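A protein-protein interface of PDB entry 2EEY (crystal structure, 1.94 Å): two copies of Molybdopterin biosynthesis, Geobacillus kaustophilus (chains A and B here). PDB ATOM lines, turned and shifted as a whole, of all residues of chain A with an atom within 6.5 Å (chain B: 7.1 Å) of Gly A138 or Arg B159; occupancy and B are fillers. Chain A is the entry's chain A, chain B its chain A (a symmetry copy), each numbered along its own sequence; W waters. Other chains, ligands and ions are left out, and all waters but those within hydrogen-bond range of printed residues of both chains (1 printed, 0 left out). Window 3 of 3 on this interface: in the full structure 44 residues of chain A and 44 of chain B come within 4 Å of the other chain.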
ATOM      1  N   THR A  35      32.546   3.985  -8.173  1.00  0.00           N
ATOM      2  CA  THR A  35      31.361   3.829  -9.005  1.00  0.00           C
ATOM      3  C   THR A  35      30.223   4.444  -8.212  1.00  0.00           C
ATOM      4  O   THR A  35      30.001   4.094  -7.053  1.00  0.00           O
ATOM      5  CB  THR A  35      31.089   2.348  -9.305  1.00  0.00           C
ATOM      6  OG1 THR A  35      32.187   1.819 -10.058  1.00  0.00           O
ATOM      7  CG2 THR A  35      29.810   2.186 -10.110  1.00  0.00           C
ATOM      8  N   VAL A  36      29.509   5.373  -8.838  1.00  0.00           N
ATOM      9  CA  VAL A  36      28.437   6.089  -8.162  1.00  0.00           C
ATOM     10  C   VAL A  36      27.093   6.045  -8.883  1.00  0.00           C
ATOM     11  O   VAL A  36      27.014   5.668 -10.047  1.00  0.00           O
ATOM     12  CB  VAL A  36      28.831   7.573  -7.984  1.00  0.00           C
ATOM     13  CG1 VAL A  36      30.173   7.676  -7.267  1.00  0.00           C
ATOM     14  CG2 VAL A  36      28.922   8.250  -9.351  1.00  0.00           C
ATOM     15  N   TYR A 129      33.959   9.273  -1.461  1.00  0.00           N
ATOM     16  CA  TYR A 129      32.860   8.566  -0.805  1.00  0.00           C
ATOM     17  C   TYR A 129      32.316   9.385   0.369  1.00  0.00           C
ATOM     18  O   TYR A 129      31.103   9.546   0.513  1.00  0.00           O
ATOM     19  CB  TYR A 129      33.331   7.182  -0.317  1.00  0.00           C
ATOM     20  CG  TYR A 129      32.240   6.328   0.305  1.00  0.00           C
ATOM     21  CD1 TYR A 129      31.689   6.659   1.543  1.00  0.00           C
ATOM     22  CD2 TYR A 129      31.729   5.212  -0.363  1.00  0.00           C
ATOM     23  CE1 TYR A 129      30.657   5.910   2.100  1.00  0.00           C
ATOM     24  CE2 TYR A 129      30.687   4.450   0.192  1.00  0.00           C
ATOM     25  CZ  TYR A 129      30.160   4.812   1.420  1.00  0.00           C
ATOM     26  OH  TYR A 129      29.120   4.095   1.973  1.00  0.00           O
ATOM     27  N   ASP A 136      24.097   8.829  -1.327  1.00  0.00           N
ATOM     28  CA  ASP A 136      23.957   7.387  -1.498  1.00  0.00           C
ATOM     29  C   ASP A 136      25.105   6.636  -0.823  1.00  0.00           C
ATOM     30  O   ASP A 136      26.269   7.005  -0.977  1.00  0.00           O
ATOM     31  CB  ASP A 136      23.940   7.042  -2.989  1.00  0.00           C
ATOM     32  CG  ASP A 136      23.513   5.613  -3.253  1.00  0.00           C
ATOM     33  OD1 ASP A 136      22.314   5.313  -3.078  1.00  0.00           O
ATOM     34  OD2 ASP A 136      24.370   4.786  -3.627  1.00  0.00           O
ATOM     35  N   LYS A 137      24.776   5.581  -0.084  1.00  0.00           N
ATOM     36  CA  LYS A 137      25.788   4.784   0.608  1.00  0.00           C
ATOM     37  C   LYS A 137      26.232   3.570  -0.200  1.00  0.00           C
ATOM     38  O   LYS A 137      27.135   2.836   0.213  1.00  0.00           O
ATOM     39  CB  LYS A 137      25.262   4.310   1.965  1.00  0.00           C
ATOM     40  CG  LYS A 137      25.455   5.294   3.107  1.00  0.00           C
ATOM     41  CD  LYS A 137      24.657   6.567   2.912  1.00  0.00           C
ATOM     42  CE  LYS A 137      24.831   7.497   4.105  1.00  0.00           C
ATOM     43  NZ  LYS A 137      24.023   8.741   3.969  1.00  0.00           N
ATOM     44  N   GLY A 138      25.606   3.368  -1.357  1.00  0.00           N
ATOM     45  CA  GLY A 138      25.940   2.229  -2.193  1.00  0.00           C
ATOM     46  C   GLY A 138      27.148   2.373  -3.104  1.00  0.00           C
ATOM     47  O   GLY A 138      27.426   1.473  -3.894  1.00  0.00           O
ATOM     48  N   MET A 139      27.867   3.489  -3.014  1.00  0.00           N
ATOM     49  CA  MET A 139      29.049   3.689  -3.855  1.00  0.00           C
ATOM     50  C   MET A 139      30.056   2.554  -3.661  1.00  0.00           C
ATOM     51  O   MET A 139      30.212   2.035  -2.555  1.00  0.00           O
ATOM     52  CB  MET A 139      29.741   5.014  -3.515  1.00  0.00           C
ATOM     53  CG  MET A 139      28.980   6.270  -3.910  1.00  0.00           C
ATOM     54  SD  MET A 139      29.912   7.739  -3.424  1.00  0.00           S
ATOM     55  CE  MET A 139      29.291   7.969  -1.748  1.00  0.00           C
ATOM     56  N   VAL A 140      30.747   2.185  -4.733  1.00  0.00           N
ATOM     57  CA  VAL A 140      31.740   1.120  -4.665  1.00  0.00           C
ATOM     58  C   VAL A 140      33.125   1.640  -5.032  1.00  0.00           C
ATOM     59  O   VAL A 140      33.305   2.281  -6.062  1.00  0.00           O
ATOM     60  CB  VAL A 140      31.390  -0.040  -5.613  1.00  0.00           C
ATOM     61  CG1 VAL A 140      32.501  -1.086  -5.581  1.00  0.00           C
ATOM     62  CG2 VAL A 140      30.057  -0.665  -5.202  1.00  0.00           C
ATOM     63  N   GLN B  31      33.471  -4.008   3.687  1.00  0.00           N
ATOM     64  CA  GLN B  31      34.158  -5.165   3.150  1.00  0.00           C
ATOM     65  C   GLN B  31      35.039  -4.827   1.959  1.00  0.00           C
ATOM     66  O   GLN B  31      34.747  -3.908   1.191  1.00  0.00           O
ATOM     67  CB  GLN B  31      33.115  -6.207   2.741  1.00  0.00           C
ATOM     68  CG  GLN B  31      33.648  -7.608   2.518  1.00  0.00           C
ATOM     69  CD  GLN B  31      32.525  -8.622   2.376  1.00  0.00           C
ATOM     70  OE1 GLN B  31      31.860  -8.688   1.347  1.00  0.00           O
ATOM     71  NE2 GLN B  31      32.298  -9.403   3.425  1.00  0.00           N
ATOM     72  N   THR B 144      35.789  -2.296  -2.653  1.00  0.00           N
ATOM     73  CA  THR B 144      35.585  -1.955  -1.250  1.00  0.00           C
ATOM     74  C   THR B 144      34.223  -1.280  -1.149  1.00  0.00           C
ATOM     75  O   THR B 144      33.923  -0.355  -1.908  1.00  0.00           O
ATOM     76  CB  THR B 144      36.689  -0.986  -0.770  1.00  0.00           C
ATOM     77  OG1 THR B 144      37.968  -1.605  -0.952  1.00  0.00           O
ATOM     78  CG2 THR B 144      36.500  -0.623   0.696  1.00  0.00           C
ATOM     79  N   TYR B 145      33.397  -1.720  -0.208  1.00  0.00           N
ATOM     80  CA  TYR B 145      32.059  -1.155  -0.087  1.00  0.00           C
ATOM     81  C   TYR B 145      31.463  -1.352   1.293  1.00  0.00           C
ATOM     82  O   TYR B 145      31.966  -2.142   2.094  1.00  0.00           O
ATOM     83  CB  TYR B 145      31.150  -1.804  -1.138  1.00  0.00           C
ATOM     84  CG  TYR B 145      31.263  -3.314  -1.143  1.00  0.00           C
ATOM     85  CD1 TYR B 145      30.531  -4.096  -0.249  1.00  0.00           C
ATOM     86  CD2 TYR B 145      32.170  -3.955  -1.988  1.00  0.00           C
ATOM     87  CE1 TYR B 145      30.707  -5.482  -0.192  1.00  0.00           C
ATOM     88  CE2 TYR B 145      32.355  -5.335  -1.938  1.00  0.00           C
ATOM     89  CZ  TYR B 145      31.624  -6.090  -1.037  1.00  0.00           C
ATOM     90  OH  TYR B 145      31.840  -7.448  -0.966  1.00  0.00           O
ATOM     91  N   LEU B 146      30.385  -0.628   1.563  1.00  0.00           N
ATOM     92  CA  LEU B 146      29.701  -0.717   2.846  1.00  0.00           C
ATOM     93  C   LEU B 146      28.742  -1.902   2.787  1.00  0.00           C
ATOM     94  O   LEU B 146      28.003  -2.066   1.813  1.00  0.00           O
ATOM     95  CB  LEU B 146      28.919   0.575   3.118  1.00  0.00           C
ATOM     96  CG  LEU B 146      28.270   0.749   4.497  1.00  0.00           C
ATOM     97  CD1 LEU B 146      29.351   0.891   5.571  1.00  0.00           C
ATOM     98  CD2 LEU B 146      27.387   1.991   4.492  1.00  0.00           C
ATOM     99  N   VAL B 147      28.765  -2.734   3.821  1.00  0.00           N
ATOM    100  CA  VAL B 147      27.890  -3.898   3.881  1.00  0.00           C
ATOM    101  C   VAL B 147      26.600  -3.514   4.595  1.00  0.00           C
ATOM    102  O   VAL B 147      25.505  -3.888   4.165  1.00  0.00           O
ATOM    103  CB  VAL B 147      28.569  -5.069   4.629  1.00  0.00           C
ATOM    104  CG1 VAL B 147      27.579  -6.216   4.817  1.00  0.00           C
ATOM    105  CG2 VAL B 147      29.783  -5.548   3.840  1.00  0.00           C
ATOM    106  N   GLU B 148      26.733  -2.757   5.681  1.00  0.00           N
ATOM    107  CA  GLU B 148      25.571  -2.308   6.433  1.00  0.00           C
ATOM    108  C   GLU B 148      25.950  -1.305   7.515  1.00  0.00           C
ATOM    109  O   GLU B 148      27.120  -1.166   7.879  1.00  0.00           O
ATOM    110  CB  GLU B 148      24.844  -3.500   7.070  1.00  0.00           C
ATOM    111  CG  GLU B 148      25.531  -4.096   8.284  1.00  0.00           C
ATOM    112  CD  GLU B 148      24.687  -5.168   8.962  1.00  0.00           C
ATOM    113  OE1 GLU B 148      23.510  -4.891   9.277  1.00  0.00           O
ATOM    114  OE2 GLU B 148      25.203  -6.285   9.184  1.00  0.00           O
ATOM    115  N   LYS B 149      24.950  -0.586   8.008  1.00  0.00           N
ATOM    116  CA  LYS B 149      25.156   0.388   9.066  1.00  0.00           C
ATOM    117  C   LYS B 149      23.847   0.526   9.832  1.00  0.00           C
ATOM    118  O   LYS B 149      22.763   0.434   9.251  1.00  0.00           O
ATOM    119  CB  LYS B 149      25.572   1.742   8.492  1.00  0.00           C
ATOM    120  CG  LYS B 149      24.447   2.511   7.829  1.00  0.00           C
ATOM    121  CD  LYS B 149      24.845   3.952   7.567  1.00  0.00           C
ATOM    122  CE  LYS B 149      23.648   4.763   7.082  1.00  0.00           C
ATOM    123  NZ  LYS B 149      22.545   4.782   8.091  1.00  0.00           N
ATOM    124  N   TYR B 157      20.819   0.496   7.023  1.00  0.00           N
ATOM    125  CA  TYR B 157      21.220   0.308   5.632  1.00  0.00           C
ATOM    126  C   TYR B 157      21.804  -1.090   5.489  1.00  0.00           C
ATOM    127  O   TYR B 157      22.479  -1.582   6.393  1.00  0.00           O
ATOM    128  CB  TYR B 157      22.282   1.329   5.217  1.00  0.00           C
ATOM    129  CG  TYR B 157      22.908   1.016   3.874  1.00  0.00           C
ATOM    130  CD1 TYR B 157      22.223   1.266   2.686  1.00  0.00           C
ATOM    131  CD2 TYR B 157      24.168   0.421   3.794  1.00  0.00           C
ATOM    132  CE1 TYR B 157      22.776   0.929   1.449  1.00  0.00           C
ATOM    133  CE2 TYR B 157      24.729   0.079   2.564  1.00  0.00           C
ATOM    134  CZ  TYR B 157      24.026   0.335   1.396  1.00  0.00           C
ATOM    135  OH  TYR B 157      24.571  -0.012   0.180  1.00  0.00           O
ATOM    136  N   ARG B 158      21.557  -1.724   4.350  1.00  0.00           N
ATOM    137  CA  ARG B 158      22.077  -3.063   4.122  1.00  0.00           C
ATOM    138  C   ARG B 158      22.155  -3.373   2.634  1.00  0.00           C
ATOM    139  O   ARG B 158      21.131  -3.498   1.962  1.00  0.00           O
ATOM    140  CB  ARG B 158      21.191  -4.086   4.832  1.00  0.00           C
ATOM    141  CG  ARG B 158      21.846  -5.438   5.034  1.00  0.00           C
ATOM    142  CD  ARG B 158      21.136  -6.210   6.130  1.00  0.00           C
ATOM    143  NE  ARG B 158      21.893  -7.382   6.555  1.00  0.00           N
ATOM    144  CZ  ARG B 158      21.602  -8.106   7.631  1.00  0.00           C
ATOM    145  NH1 ARG B 158      20.566  -7.776   8.391  1.00  0.00           N
ATOM    146  NH2 ARG B 158      22.347  -9.158   7.948  1.00  0.00           N
ATOM    147  N   ARG B 159      23.377  -3.487   2.123  1.00  0.00           N
ATOM    148  CA  ARG B 159      23.592  -3.783   0.714  1.00  0.00           C
ATOM    149  C   ARG B 159      22.877  -5.065   0.307  1.00  0.00           C
ATOM    150  O   ARG B 159      23.013  -6.101   0.958  1.00  0.00           O
ATOM    151  CB  ARG B 159      25.090  -3.907   0.419  1.00  0.00           C
ATOM    152  CG  ARG B 159      25.413  -4.428  -0.974  1.00  0.00           C
ATOM    153  CD  ARG B 159      26.910  -4.414  -1.231  1.00  0.00           C
ATOM    154  NE  ARG B 159      27.416  -3.054  -1.385  1.00  0.00           N
ATOM    155  CZ  ARG B 159      27.231  -2.307  -2.470  1.00  0.00           C
ATOM    156  NH1 ARG B 159      26.558  -2.792  -3.504  1.00  0.00           N
ATOM    157  NH2 ARG B 159      27.711  -1.072  -2.519  1.00  0.00           N
ATOM    158  N   LYS B 160      22.108  -4.983  -0.774  1.00  0.00           N
ATOM    159  CA  LYS B 160      21.367  -6.129  -1.282  1.00  0.00           C
ATOM    160  C   LYS B 160      22.312  -7.122  -1.953  1.00  0.00           C
ATOM    161  O   LYS B 160      23.249  -6.729  -2.649  1.00  0.00           O
ATOM    162  CB  LYS B 160      20.304  -5.669  -2.285  1.00  0.00           C
ATOM    163  CG  LYS B 160      20.853  -4.955  -3.520  1.00  0.00           C
ATOM    164  CD  LYS B 160      21.586  -3.668  -3.159  1.00  0.00           C
ATOM    165  CE  LYS B 160      20.684  -2.710  -2.392  1.00  0.00           C
ATOM    166  NZ  LYS B 160      21.419  -1.508  -1.918  1.00  0.00           N
ATOM    167  N   THR B 161      22.060  -8.408  -1.735  1.00  0.00           N
ATOM    168  CA  THR B 161      22.884  -9.462  -2.315  1.00  0.00           C
ATOM    169  C   THR B 161      22.019 -10.561  -2.925  1.00  0.00           C
ATOM    170  O   THR B 161      20.778 -10.442  -2.847  1.00  0.00           O
ATOM    171  CB  THR B 161      23.810 -10.095  -1.253  1.00  0.00           C
ATOM    172  OG1 THR B 161      23.020 -10.612  -0.175  1.00  0.00           O
ATOM    173  CG2 THR B 161      24.784  -9.060  -0.711  1.00  0.00           C
HETATM  174  O   HOH W   1      29.163   1.155  -0.344  1.00  0.00           O
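Water W1 lies within hydrogen-bond range of O of Met A139 (2.6 Å), O of Lys A137 (2.7 Å), N of Leu B146 (2.9 Å) and NH2 of Arg B159 (3.4 Å).
The backbone carbonyl oxygen (O) of Gly A138 lies within hydrogen-bond range of the guanidinium group (NH2) of Arg B159, 2.9 Å away.
No position is printed for both chains.
Printed residues of chain B within 4 Å of Tyr A129: Leu B146 (3.7 Å).
Of chain B, only Tyr B157 and Arg B159 come within 4 Å of Gly A138.
Of the printed residues of chain B, Met A139 touches Arg B159.
Of the printed residues of chain B, Val A140 touches Thr B144 (3.8 Å) and Arg B159 (3.6 Å).
Printed residues of chain A within 4 Å of Arg B159: Gly A138 (2.9 Å), Met A139 (3.99 Å) and Val A140 (3.6 Å).
Thr B161 touches none of the printed residues of chain A.
The nearest printed residue of chain A that does not touch Arg B159 is Lys A137 (4.8 Å).
Printed residues of chain B that touch a printed residue of chain A: Thr B144, Leu B146, Tyr B157 and Arg B159.
Hydrophobic or aromatic side chains of chain B within 4 Å of the printed part of chain A: Leu B146 and Tyr B157.
Hydrophobic or aromatic side chains of chain A within 4 Å of the printed part of chain B: Tyr A129 and Val A140.
Among the printed residues, 7 pairs touch across the chains.
Among the printed residues, merely in contact across the chains: Tyr A129 with Leu B146, Lys A137 with Tyr B157, Gly A138 with Tyr B157, Met A139 with Arg B159, Val A140 with Thr B144 and Val A140 with Arg B159.
O of Val A140 is in hydrogen-bond range of N of Thr A35 (2.8 Å).
The backbone carbonyl oxygen of Lys A137 sits at hydrogen-bond distance from the side-chain hydroxyl of Tyr A129 (2.9 Å).
The side-chain carboxylate of Asp A136 lies within hydrogen-bond range of the backbone NH of Gly A138, at 2.9 Å.
The backbone carbonyl oxygen (O) of Leu B146 lies within hydrogen-bond range of the guanidinium group (NE) of Arg B159 (3.4 Å).
The backbone carbonyl oxygen (O) of Val B147 sits at hydrogen-bond distance from the backbone NH (N) of Arg B159.
The backbone carbonyl oxygen (O) of Lys B149 lies within hydrogen-bond range of the backbone NH (N) of Tyr B157.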
